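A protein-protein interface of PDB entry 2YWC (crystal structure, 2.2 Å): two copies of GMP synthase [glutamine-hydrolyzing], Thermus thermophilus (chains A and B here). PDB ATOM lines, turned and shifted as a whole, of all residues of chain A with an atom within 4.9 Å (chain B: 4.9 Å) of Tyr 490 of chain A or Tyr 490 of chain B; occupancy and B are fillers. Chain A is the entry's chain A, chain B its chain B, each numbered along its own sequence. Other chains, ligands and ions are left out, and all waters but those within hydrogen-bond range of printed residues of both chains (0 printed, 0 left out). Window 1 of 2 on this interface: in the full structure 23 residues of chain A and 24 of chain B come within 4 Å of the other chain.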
ATOM      1  N   LEU A 450       7.244  -9.924  22.073  1.00  0.00           N
ATOM      2  CA  LEU A 450       5.916 -10.448  21.791  1.00  0.00           C
ATOM      3  C   LEU A 450       4.977  -9.293  22.114  1.00  0.00           C
ATOM      4  O   LEU A 450       5.212  -8.524  23.062  1.00  0.00           O
ATOM      5  CB  LEU A 450       5.615 -11.677  22.651  1.00  0.00           C
ATOM      6  CG  LEU A 450       6.473 -12.889  22.283  1.00  0.00           C
ATOM      7  CD1 LEU A 450       6.035 -14.101  23.083  1.00  0.00           C
ATOM      8  CD2 LEU A 450       6.334 -13.157  20.785  1.00  0.00           C
ATOM      9  N   ARG A 451       3.911  -9.178  21.337  1.00  0.00           N
ATOM     10  CA  ARG A 451       2.996  -8.064  21.485  1.00  0.00           C
ATOM     11  C   ARG A 451       1.584  -8.435  21.033  1.00  0.00           C
ATOM     12  O   ARG A 451       1.380  -8.903  19.907  1.00  0.00           O
ATOM     13  CB  ARG A 451       3.571  -6.913  20.649  1.00  0.00           C
ATOM     14  CG  ARG A 451       2.653  -5.785  20.216  1.00  0.00           C
ATOM     15  CD  ARG A 451       2.281  -5.046  21.503  1.00  0.00           C
ATOM     16  NE  ARG A 451       1.973  -3.653  21.252  1.00  0.00           N
ATOM     17  CZ  ARG A 451       1.604  -2.833  22.224  1.00  0.00           C
ATOM     18  NH1 ARG A 451       1.508  -3.315  23.460  1.00  0.00           N
ATOM     19  NH2 ARG A 451       1.352  -1.555  21.977  1.00  0.00           N
ATOM     20  N   ALA A 452       0.620  -8.252  21.929  1.00  0.00           N
ATOM     21  CA  ALA A 452      -0.778  -8.542  21.634  1.00  0.00           C
ATOM     22  C   ALA A 452      -1.628  -7.496  22.350  1.00  0.00           C
ATOM     23  O   ALA A 452      -1.281  -7.039  23.448  1.00  0.00           O
ATOM     24  CB  ALA A 452      -1.142  -9.950  22.099  1.00  0.00           C
ATOM     25  N   TRP A 463      -2.826  -3.471  26.294  1.00  0.00           N
ATOM     26  CA  TRP A 463      -1.982  -4.617  26.073  1.00  0.00           C
ATOM     27  C   TRP A 463      -2.795  -5.834  26.523  1.00  0.00           C
ATOM     28  O   TRP A 463      -3.573  -5.763  27.476  1.00  0.00           O
ATOM     29  CB  TRP A 463      -0.653  -4.476  26.813  1.00  0.00           C
ATOM     30  CG  TRP A 463      -0.727  -4.340  28.294  1.00  0.00           C
ATOM     31  CD1 TRP A 463      -1.012  -3.213  29.005  1.00  0.00           C
ATOM     32  CD2 TRP A 463      -0.450  -5.368  29.258  1.00  0.00           C
ATOM     33  NE1 TRP A 463      -0.922  -3.474  30.354  1.00  0.00           N
ATOM     34  CE2 TRP A 463      -0.578  -4.789  30.534  1.00  0.00           C
ATOM     35  CE3 TRP A 463      -0.102  -6.724  29.158  1.00  0.00           C
ATOM     36  CZ2 TRP A 463      -0.372  -5.517  31.710  1.00  0.00           C
ATOM     37  CZ3 TRP A 463       0.104  -7.450  30.317  1.00  0.00           C
ATOM     38  CH2 TRP A 463      -0.031  -6.846  31.582  1.00  0.00           C
ATOM     39  N   ALA A 464      -2.669  -6.934  25.790  1.00  0.00           N
ATOM     40  CA  ALA A 464      -3.422  -8.130  26.113  1.00  0.00           C
ATOM     41  C   ALA A 464      -2.780  -8.818  27.311  1.00  0.00           C
ATOM     42  O   ALA A 464      -1.567  -8.996  27.357  1.00  0.00           O
ATOM     43  CB  ALA A 464      -3.458  -9.070  24.896  1.00  0.00           C
ATOM     44  N   ARG A 465      -3.585  -9.198  28.290  1.00  0.00           N
ATOM     45  CA  ARG A 465      -3.032  -9.863  29.461  1.00  0.00           C
ATOM     46  C   ARG A 465      -3.113 -11.366  29.278  1.00  0.00           C
ATOM     47  O   ARG A 465      -4.007 -12.028  29.797  1.00  0.00           O
ATOM     48  CB  ARG A 465      -3.778  -9.408  30.715  1.00  0.00           C
ATOM     49  CG  ARG A 465      -3.850  -7.890  30.769  1.00  0.00           C
ATOM     50  CD  ARG A 465      -4.169  -7.355  32.126  1.00  0.00           C
ATOM     51  NE  ARG A 465      -4.121  -5.903  32.104  1.00  0.00           N
ATOM     52  CZ  ARG A 465      -4.355  -5.133  33.160  1.00  0.00           C
ATOM     53  NH1 ARG A 465      -4.656  -5.682  34.341  1.00  0.00           N
ATOM     54  NH2 ARG A 465      -4.288  -3.809  33.029  1.00  0.00           N
ATOM     55  N   LEU A 466      -2.176 -11.890  28.500  1.00  0.00           N
ATOM     56  CA  LEU A 466      -2.115 -13.316  28.215  1.00  0.00           C
ATOM     57  C   LEU A 466      -1.643 -14.032  29.472  1.00  0.00           C
ATOM     58  O   LEU A 466      -0.862 -13.484  30.236  1.00  0.00           O
ATOM     59  CB  LEU A 466      -1.135 -13.565  27.064  1.00  0.00           C
ATOM     60  CG  LEU A 466      -1.532 -12.831  25.781  1.00  0.00           C
ATOM     61  CD1 LEU A 466      -0.397 -12.861  24.778  1.00  0.00           C
ATOM     62  CD2 LEU A 466      -2.802 -13.494  25.217  1.00  0.00           C
ATOM     63  N   LEU A 471       2.774 -17.224  28.321  1.00  0.00           N
ATOM     64  CA  LEU A 471       3.937 -16.426  27.962  1.00  0.00           C
ATOM     65  C   LEU A 471       5.225 -17.229  28.181  1.00  0.00           C
ATOM     66  O   LEU A 471       6.165 -17.136  27.396  1.00  0.00           O
ATOM     67  CB  LEU A 471       3.956 -15.118  28.775  1.00  0.00           C
ATOM     68  CG  LEU A 471       2.802 -14.160  28.420  1.00  0.00           C
ATOM     69  CD1 LEU A 471       2.879 -12.863  29.231  1.00  0.00           C
ATOM     70  CD2 LEU A 471       2.872 -13.840  26.945  1.00  0.00           C
ATOM     71  N   VAL A 488      13.403 -13.180  25.052  1.00  0.00           N
ATOM     72  CA  VAL A 488      12.030 -12.860  24.671  1.00  0.00           C
ATOM     73  C   VAL A 488      11.372 -11.981  25.731  1.00  0.00           C
ATOM     74  O   VAL A 488      11.490 -12.246  26.930  1.00  0.00           O
ATOM     75  CB  VAL A 488      11.202 -14.152  24.473  1.00  0.00           C
ATOM     76  CG1 VAL A 488       9.734 -13.840  24.281  1.00  0.00           C
ATOM     77  CG2 VAL A 488      11.728 -14.891  23.254  1.00  0.00           C
ATOM     78  N   VAL A 489      10.693 -10.925  25.280  1.00  0.00           N
ATOM     79  CA  VAL A 489      10.003  -9.999  26.178  1.00  0.00           C
ATOM     80  C   VAL A 489       8.579  -9.771  25.724  1.00  0.00           C
ATOM     81  O   VAL A 489       8.241  -9.980  24.560  1.00  0.00           O
ATOM     82  CB  VAL A 489      10.683  -8.593  26.248  1.00  0.00           C
ATOM     83  CG1 VAL A 489      12.116  -8.726  26.720  1.00  0.00           C
ATOM     84  CG2 VAL A 489      10.619  -7.891  24.866  1.00  0.00           C
ATOM     85  N   TYR A 490       7.745  -9.336  26.658  1.00  0.00           N
ATOM     86  CA  TYR A 490       6.354  -9.057  26.354  1.00  0.00           C
ATOM     87  C   TYR A 490       6.085  -7.567  26.572  1.00  0.00           C
ATOM     88  O   TYR A 490       6.398  -7.017  27.623  1.00  0.00           O
ATOM     89  CB  TYR A 490       5.432  -9.905  27.236  1.00  0.00           C
ATOM     90  CG  TYR A 490       4.006  -9.848  26.775  1.00  0.00           C
ATOM     91  CD1 TYR A 490       3.667 -10.256  25.493  1.00  0.00           C
ATOM     92  CD2 TYR A 490       3.000  -9.329  27.590  1.00  0.00           C
ATOM     93  CE1 TYR A 490       2.358 -10.142  25.025  1.00  0.00           C
ATOM     94  CE2 TYR A 490       1.679  -9.213  27.128  1.00  0.00           C
ATOM     95  CZ  TYR A 490       1.368  -9.622  25.841  1.00  0.00           C
ATOM     96  OH  TYR A 490       0.074  -9.514  25.354  1.00  0.00           O
ATOM     97  N   ASP A 491       5.507  -6.925  25.566  1.00  0.00           N
ATOM     98  CA  ASP A 491       5.205  -5.498  25.614  1.00  0.00           C
ATOM     99  C   ASP A 491       4.053  -5.198  26.584  1.00  0.00           C
ATOM    100  O   ASP A 491       2.950  -5.746  26.441  1.00  0.00           O
ATOM    101  CB  ASP A 491       4.836  -5.009  24.209  1.00  0.00           C
ATOM    102  CG  ASP A 491       4.853  -3.499  24.095  1.00  0.00           C
ATOM    103  OD1 ASP A 491       4.654  -2.817  25.128  1.00  0.00           O
ATOM    104  OD2 ASP A 491       5.054  -2.998  22.970  1.00  0.00           O
ATOM    105  N   LEU A 492       4.298  -4.322  27.556  1.00  0.00           N
ATOM    106  CA  LEU A 492       3.275  -3.983  28.543  1.00  0.00           C
ATOM    107  C   LEU A 492       2.607  -2.619  28.306  1.00  0.00           C
ATOM    108  O   LEU A 492       1.843  -2.135  29.144  1.00  0.00           O
ATOM    109  CB  LEU A 492       3.889  -3.985  29.937  1.00  0.00           C
ATOM    110  CG  LEU A 492       4.537  -5.283  30.422  1.00  0.00           C
ATOM    111  CD1 LEU A 492       5.293  -5.012  31.710  1.00  0.00           C
ATOM    112  CD2 LEU A 492       3.462  -6.352  30.621  1.00  0.00           C
ATOM    113  N   LEU B 450      11.705  -4.376  32.044  1.00  0.00           N
ATOM    114  CA  LEU B 450      11.641  -4.733  33.458  1.00  0.00           C
ATOM    115  C   LEU B 450      12.103  -6.178  33.537  1.00  0.00           C
ATOM    116  O   LEU B 450      11.814  -6.988  32.648  1.00  0.00           O
ATOM    117  CB  LEU B 450      10.219  -4.580  33.995  1.00  0.00           C
ATOM    118  CG  LEU B 450       9.745  -3.128  34.100  1.00  0.00           C
ATOM    119  CD1 LEU B 450       8.362  -3.081  34.730  1.00  0.00           C
ATOM    120  CD2 LEU B 450      10.722  -2.343  34.948  1.00  0.00           C
ATOM    121  N   ARG B 451      12.821  -6.503  34.600  1.00  0.00           N
ATOM    122  CA  ARG B 451      13.374  -7.835  34.737  1.00  0.00           C
ATOM    123  C   ARG B 451      13.477  -8.280  36.188  1.00  0.00           C
ATOM    124  O   ARG B 451      14.163  -7.648  36.985  1.00  0.00           O
ATOM    125  CB  ARG B 451      14.752  -7.827  34.071  1.00  0.00           C
ATOM    126  CG  ARG B 451      15.700  -8.957  34.421  1.00  0.00           C
ATOM    127  CD  ARG B 451      15.173 -10.269  33.950  1.00  0.00           C
ATOM    128  NE  ARG B 451      16.232 -11.210  33.601  1.00  0.00           N
ATOM    129  CZ  ARG B 451      15.980 -12.429  33.138  1.00  0.00           C
ATOM    130  NH1 ARG B 451      14.711 -12.815  32.995  1.00  0.00           N
ATOM    131  NH2 ARG B 451      16.970 -13.242  32.798  1.00  0.00           N
ATOM    132  N   ALA B 452      12.788  -9.371  36.525  1.00  0.00           N
ATOM    133  CA  ALA B 452      12.824  -9.918  37.879  1.00  0.00           C
ATOM    134  C   ALA B 452      12.894 -11.437  37.821  1.00  0.00           C
ATOM    135  O   ALA B 452      12.306 -12.060  36.935  1.00  0.00           O
ATOM    136  CB  ALA B 452      11.599  -9.483  38.656  1.00  0.00           C
ATOM    137  N   TRP B 463      12.197 -16.592  35.469  1.00  0.00           N
ATOM    138  CA  TRP B 463      11.690 -15.239  35.371  1.00  0.00           C
ATOM    139  C   TRP B 463      10.537 -15.203  36.352  1.00  0.00           C
ATOM    140  O   TRP B 463       9.736 -16.128  36.416  1.00  0.00           O
ATOM    141  CB  TRP B 463      11.244 -14.895  33.937  1.00  0.00           C
ATOM    142  CG  TRP B 463      10.121 -15.716  33.371  1.00  0.00           C
ATOM    143  CD1 TRP B 463      10.216 -16.942  32.774  1.00  0.00           C
ATOM    144  CD2 TRP B 463       8.737 -15.341  33.304  1.00  0.00           C
ATOM    145  NE1 TRP B 463       8.977 -17.352  32.331  1.00  0.00           N
ATOM    146  CE2 TRP B 463       8.051 -16.392  32.643  1.00  0.00           C
ATOM    147  CE3 TRP B 463       8.012 -14.221  33.727  1.00  0.00           C
ATOM    148  CZ2 TRP B 463       6.665 -16.353  32.397  1.00  0.00           C
ATOM    149  CZ3 TRP B 463       6.621 -14.175  33.476  1.00  0.00           C
ATOM    150  CH2 TRP B 463       5.971 -15.236  32.821  1.00  0.00           C
ATOM    151  N   ALA B 464      10.476 -14.146  37.146  1.00  0.00           N
ATOM    152  CA  ALA B 464       9.439 -14.025  38.158  1.00  0.00           C
ATOM    153  C   ALA B 464       8.057 -13.771  37.553  1.00  0.00           C
ATOM    154  O   ALA B 464       7.890 -12.876  36.722  1.00  0.00           O
ATOM    155  CB  ALA B 464       9.818 -12.911  39.145  1.00  0.00           C
ATOM    156  N   ARG B 465       7.078 -14.577  37.970  1.00  0.00           N
ATOM    157  CA  ARG B 465       5.704 -14.453  37.485  1.00  0.00           C
ATOM    158  C   ARG B 465       4.973 -13.334  38.263  1.00  0.00           C
ATOM    159  O   ARG B 465       4.046 -13.589  39.025  1.00  0.00           O
ATOM    160  CB  ARG B 465       4.936 -15.785  37.658  1.00  0.00           C
ATOM    161  CG  ARG B 465       5.688 -17.074  37.240  1.00  0.00           C
ATOM    162  CD  ARG B 465       6.257 -16.985  35.844  1.00  0.00           C
ATOM    163  NE  ARG B 465       6.827 -18.242  35.348  1.00  0.00           N
ATOM    164  CZ  ARG B 465       6.126 -19.342  35.074  1.00  0.00           C
ATOM    165  NH1 ARG B 465       4.847 -19.455  35.448  1.00  0.00           N
ATOM    166  NH2 ARG B 465       6.695 -20.326  34.386  1.00  0.00           N
ATOM    167  N   LEU B 466       5.401 -12.096  38.074  1.00  0.00           N
ATOM    168  CA  LEU B 466       4.759 -10.981  38.752  1.00  0.00           C
ATOM    169  C   LEU B 466       3.302 -10.852  38.303  1.00  0.00           C
ATOM    170  O   LEU B 466       2.959 -11.205  37.172  1.00  0.00           O
ATOM    171  CB  LEU B 466       5.521  -9.693  38.446  1.00  0.00           C
ATOM    172  CG  LEU B 466       6.968  -9.730  38.965  1.00  0.00           C
ATOM    173  CD1 LEU B 466       7.714  -8.472  38.540  1.00  0.00           C
ATOM    174  CD2 LEU B 466       6.953  -9.870  40.491  1.00  0.00           C
ATOM    175  N   LEU B 471       2.335  -5.331  36.759  1.00  0.00           N
ATOM    176  CA  LEU B 471       3.171  -4.921  35.644  1.00  0.00           C
ATOM    177  C   LEU B 471       2.526  -3.761  34.896  1.00  0.00           C
ATOM    178  O   LEU B 471       3.220  -2.910  34.345  1.00  0.00           O
ATOM    179  CB  LEU B 471       3.405  -6.105  34.698  1.00  0.00           C
ATOM    180  CG  LEU B 471       4.158  -7.295  35.323  1.00  0.00           C
ATOM    181  CD1 LEU B 471       4.040  -8.528  34.405  1.00  0.00           C
ATOM    182  CD2 LEU B 471       5.610  -6.913  35.553  1.00  0.00           C
ATOM    183  N   VAL B 488       7.425   0.150  27.716  1.00  0.00           N
ATOM    184  CA  VAL B 488       7.908  -0.693  28.798  1.00  0.00           C
ATOM    185  C   VAL B 488       7.647  -2.152  28.449  1.00  0.00           C
ATOM    186  O   VAL B 488       6.550  -2.530  28.030  1.00  0.00           O
ATOM    187  CB  VAL B 488       7.233  -0.344  30.128  1.00  0.00           C
ATOM    188  CG1 VAL B 488       7.766  -1.258  31.242  1.00  0.00           C
ATOM    189  CG2 VAL B 488       7.507   1.121  30.461  1.00  0.00           C
ATOM    190  N   VAL B 489       8.667  -2.968  28.666  1.00  0.00           N
ATOM    191  CA  VAL B 489       8.641  -4.382  28.334  1.00  0.00           C
ATOM    192  C   VAL B 489       8.986  -5.265  29.552  1.00  0.00           C
ATOM    193  O   VAL B 489       9.626  -4.795  30.482  1.00  0.00           O
ATOM    194  CB  VAL B 489       9.667  -4.591  27.199  1.00  0.00           C
ATOM    195  CG1 VAL B 489      10.598  -5.704  27.530  1.00  0.00           C
ATOM    196  CG2 VAL B 489       8.971  -4.778  25.884  1.00  0.00           C
ATOM    197  N   TYR B 490       8.548  -6.528  29.554  1.00  0.00           N
ATOM    198  CA  TYR B 490       8.877  -7.440  30.654  1.00  0.00           C
ATOM    199  C   TYR B 490       9.585  -8.685  30.122  1.00  0.00           C
ATOM    200  O   TYR B 490       9.101  -9.340  29.205  1.00  0.00           O
ATOM    201  CB  TYR B 490       7.636  -7.856  31.459  1.00  0.00           C
ATOM    202  CG  TYR B 490       8.013  -8.579  32.751  1.00  0.00           C
ATOM    203  CD1 TYR B 490       8.874  -7.977  33.679  1.00  0.00           C
ATOM    204  CD2 TYR B 490       7.539  -9.869  33.028  1.00  0.00           C
ATOM    205  CE1 TYR B 490       9.261  -8.645  34.851  1.00  0.00           C
ATOM    206  CE2 TYR B 490       7.908 -10.545  34.201  1.00  0.00           C
ATOM    207  CZ  TYR B 490       8.775  -9.928  35.108  1.00  0.00           C
ATOM    208  OH  TYR B 490       9.171 -10.588  36.261  1.00  0.00           O
ATOM    209  N   ASP B 491      10.730  -9.001  30.712  1.00  0.00           N
ATOM    210  CA  ASP B 491      11.564 -10.134  30.288  1.00  0.00           C
ATOM    211  C   ASP B 491      10.950 -11.485  30.711  1.00  0.00           C
ATOM    212  O   ASP B 491      10.702 -11.725  31.900  1.00  0.00           O
ATOM    213  CB  ASP B 491      12.970  -9.943  30.885  1.00  0.00           C
ATOM    214  CG  ASP B 491      14.053 -10.827  30.225  1.00  0.00           C
ATOM    215  OD1 ASP B 491      15.260 -10.470  30.347  1.00  0.00           O
ATOM    216  OD2 ASP B 491      13.720 -11.868  29.619  1.00  0.00           O
ATOM    217  N   LEU B 492      10.711 -12.357  29.732  1.00  0.00           N
ATOM    218  CA  LEU B 492      10.122 -13.674  29.986  1.00  0.00           C
ATOM    219  C   LEU B 492      11.162 -14.784  29.915  1.00  0.00           C
ATOM    220  O   LEU B 492      10.805 -15.958  29.857  1.00  0.00           O
ATOM    221  CB  LEU B 492       9.044 -13.982  28.941  1.00  0.00           C
ATOM    222  CG  LEU B 492       7.946 -12.942  28.696  1.00  0.00           C
ATOM    223  CD1 LEU B 492       7.168 -13.287  27.437  1.00  0.00           C
ATOM    224  CD2 LEU B 492       7.034 -12.867  29.920  1.00  0.00           C
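O of Val 488 of chain A is in hydrogen-bond range of N of Leu 492 of chain B (2.9 Å). The backbone carbonyl oxygen of Val 488 of chain B sits close to the side-chain carboxylate of Asp 491 of chain A, at 3.5 Å. The backbone NH (N) of Leu 492 of chain A sits at hydrogen-bond distance from the backbone carbonyl oxygen (O) of Val 488 of chain B, 2.9 Å away. N of Tyr 490 of chain A sits at hydrogen-bond distance from O of Tyr 490 of chain B (2.9 Å).
The backbone carbonyl oxygen of Leu 492 of chain A lies close to the indole nitrogen of Trp 463 of chain A (3.3 Å). The side-chain hydroxyl of Tyr 490 of chain A sits at hydrogen-bond distance from the backbone carbonyl oxygen of Ala 464 of chain A (2.6 Å). N of Asp 491 of chain A is in hydrogen-bond range of O of Leu 450 of chain A (3.0 Å). NE of Arg 451 of chain A lies within salt-bridge range of OD2 of Asp 491 of chain A (3.6 Å). O of Ala 452 of chain A is in hydrogen-bond range of OH of Tyr 490 of chain A. The backbone carbonyl oxygen (O) of Leu 450 of chain B is in hydrogen-bond range of the backbone NH (N) of Asp 491 of chain B (3.0 Å).
Among the printed residues, merely in contact across the chains: Leu 471 of chain A with Leu 492 of chain B (3.9 Å), Val 488 of chain A with Asp 491 of chain B (3.5 Å), Val 489 of chain A with Val 489 of chain B (3.2 Å), Val 489 of chain A with Tyr 490 of chain B (3.2 Å), Val 489 of chain A with Asp 491 of chain B (3.9 Å), Tyr 490 of chain A with Val 489 of chain B (3.5 Å), Tyr 490 of chain A with Leu 492 of chain B (3.8 Å), Asp 491 of chain A with Val 489 of chain B (3.8 Å), Leu 492 of chain A with Leu 471 of chain B (3.7 Å) and Leu 492 of chain A with Tyr 490 of chain B (3.7 Å).
Of the printed residues of chain B, Leu 471 of chain A touches Leu 492 (3.9 Å). Tyr 490 of chain A touches three residues of chain B. Printed residues of chain B within 4 Å of Asp 491 of chain A: Val 488 (3.5 Å) and Val 489 (3.8 Å). Leu 450 of chain B touches none of the printed residues of chain A. The nearest residue of chain A that does not touch Tyr 490 of chain B is Val 488 of chain A (4.4 Å). The nearest printed residue of chain A that does not touch Asp 491 of chain B is Tyr 490 of chain A (5.0 Å).
Of the 13 printed residues of chain B, 6 touch a printed residue of chain A. Hydrophobic or aromatic side chains of chain B within 4 Å of the printed part of chain A: Leu 471, Val 489, Tyr 490 and Leu 492. Of the 13 printed residues of chain A, 6 touch a printed residue of chain B. Hydrophobic or aromatic side chains of chain A that line the printed part of chain B: Leu 471, Val 489, Tyr 490 and Leu 492. Among the printed residues, 14 pairs touch across the chains.
Val 488 of chain A touches Asp 491 of chain B, and with the chains exchanged Asp 491 of chain A touches Val 488 of chain B. Val 489 of chain A touches its own counterpart, Val 489 of chain B. Val 489 of chain A touches Asp 491 of chain B, and with the chains exchanged Asp 491 of chain A touches Val 489 of chain B. Tyr 490 of chain A touches Leu 492 of chain B, and with the chains exchanged Leu 492 of chain A touches Tyr 490 of chain B.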
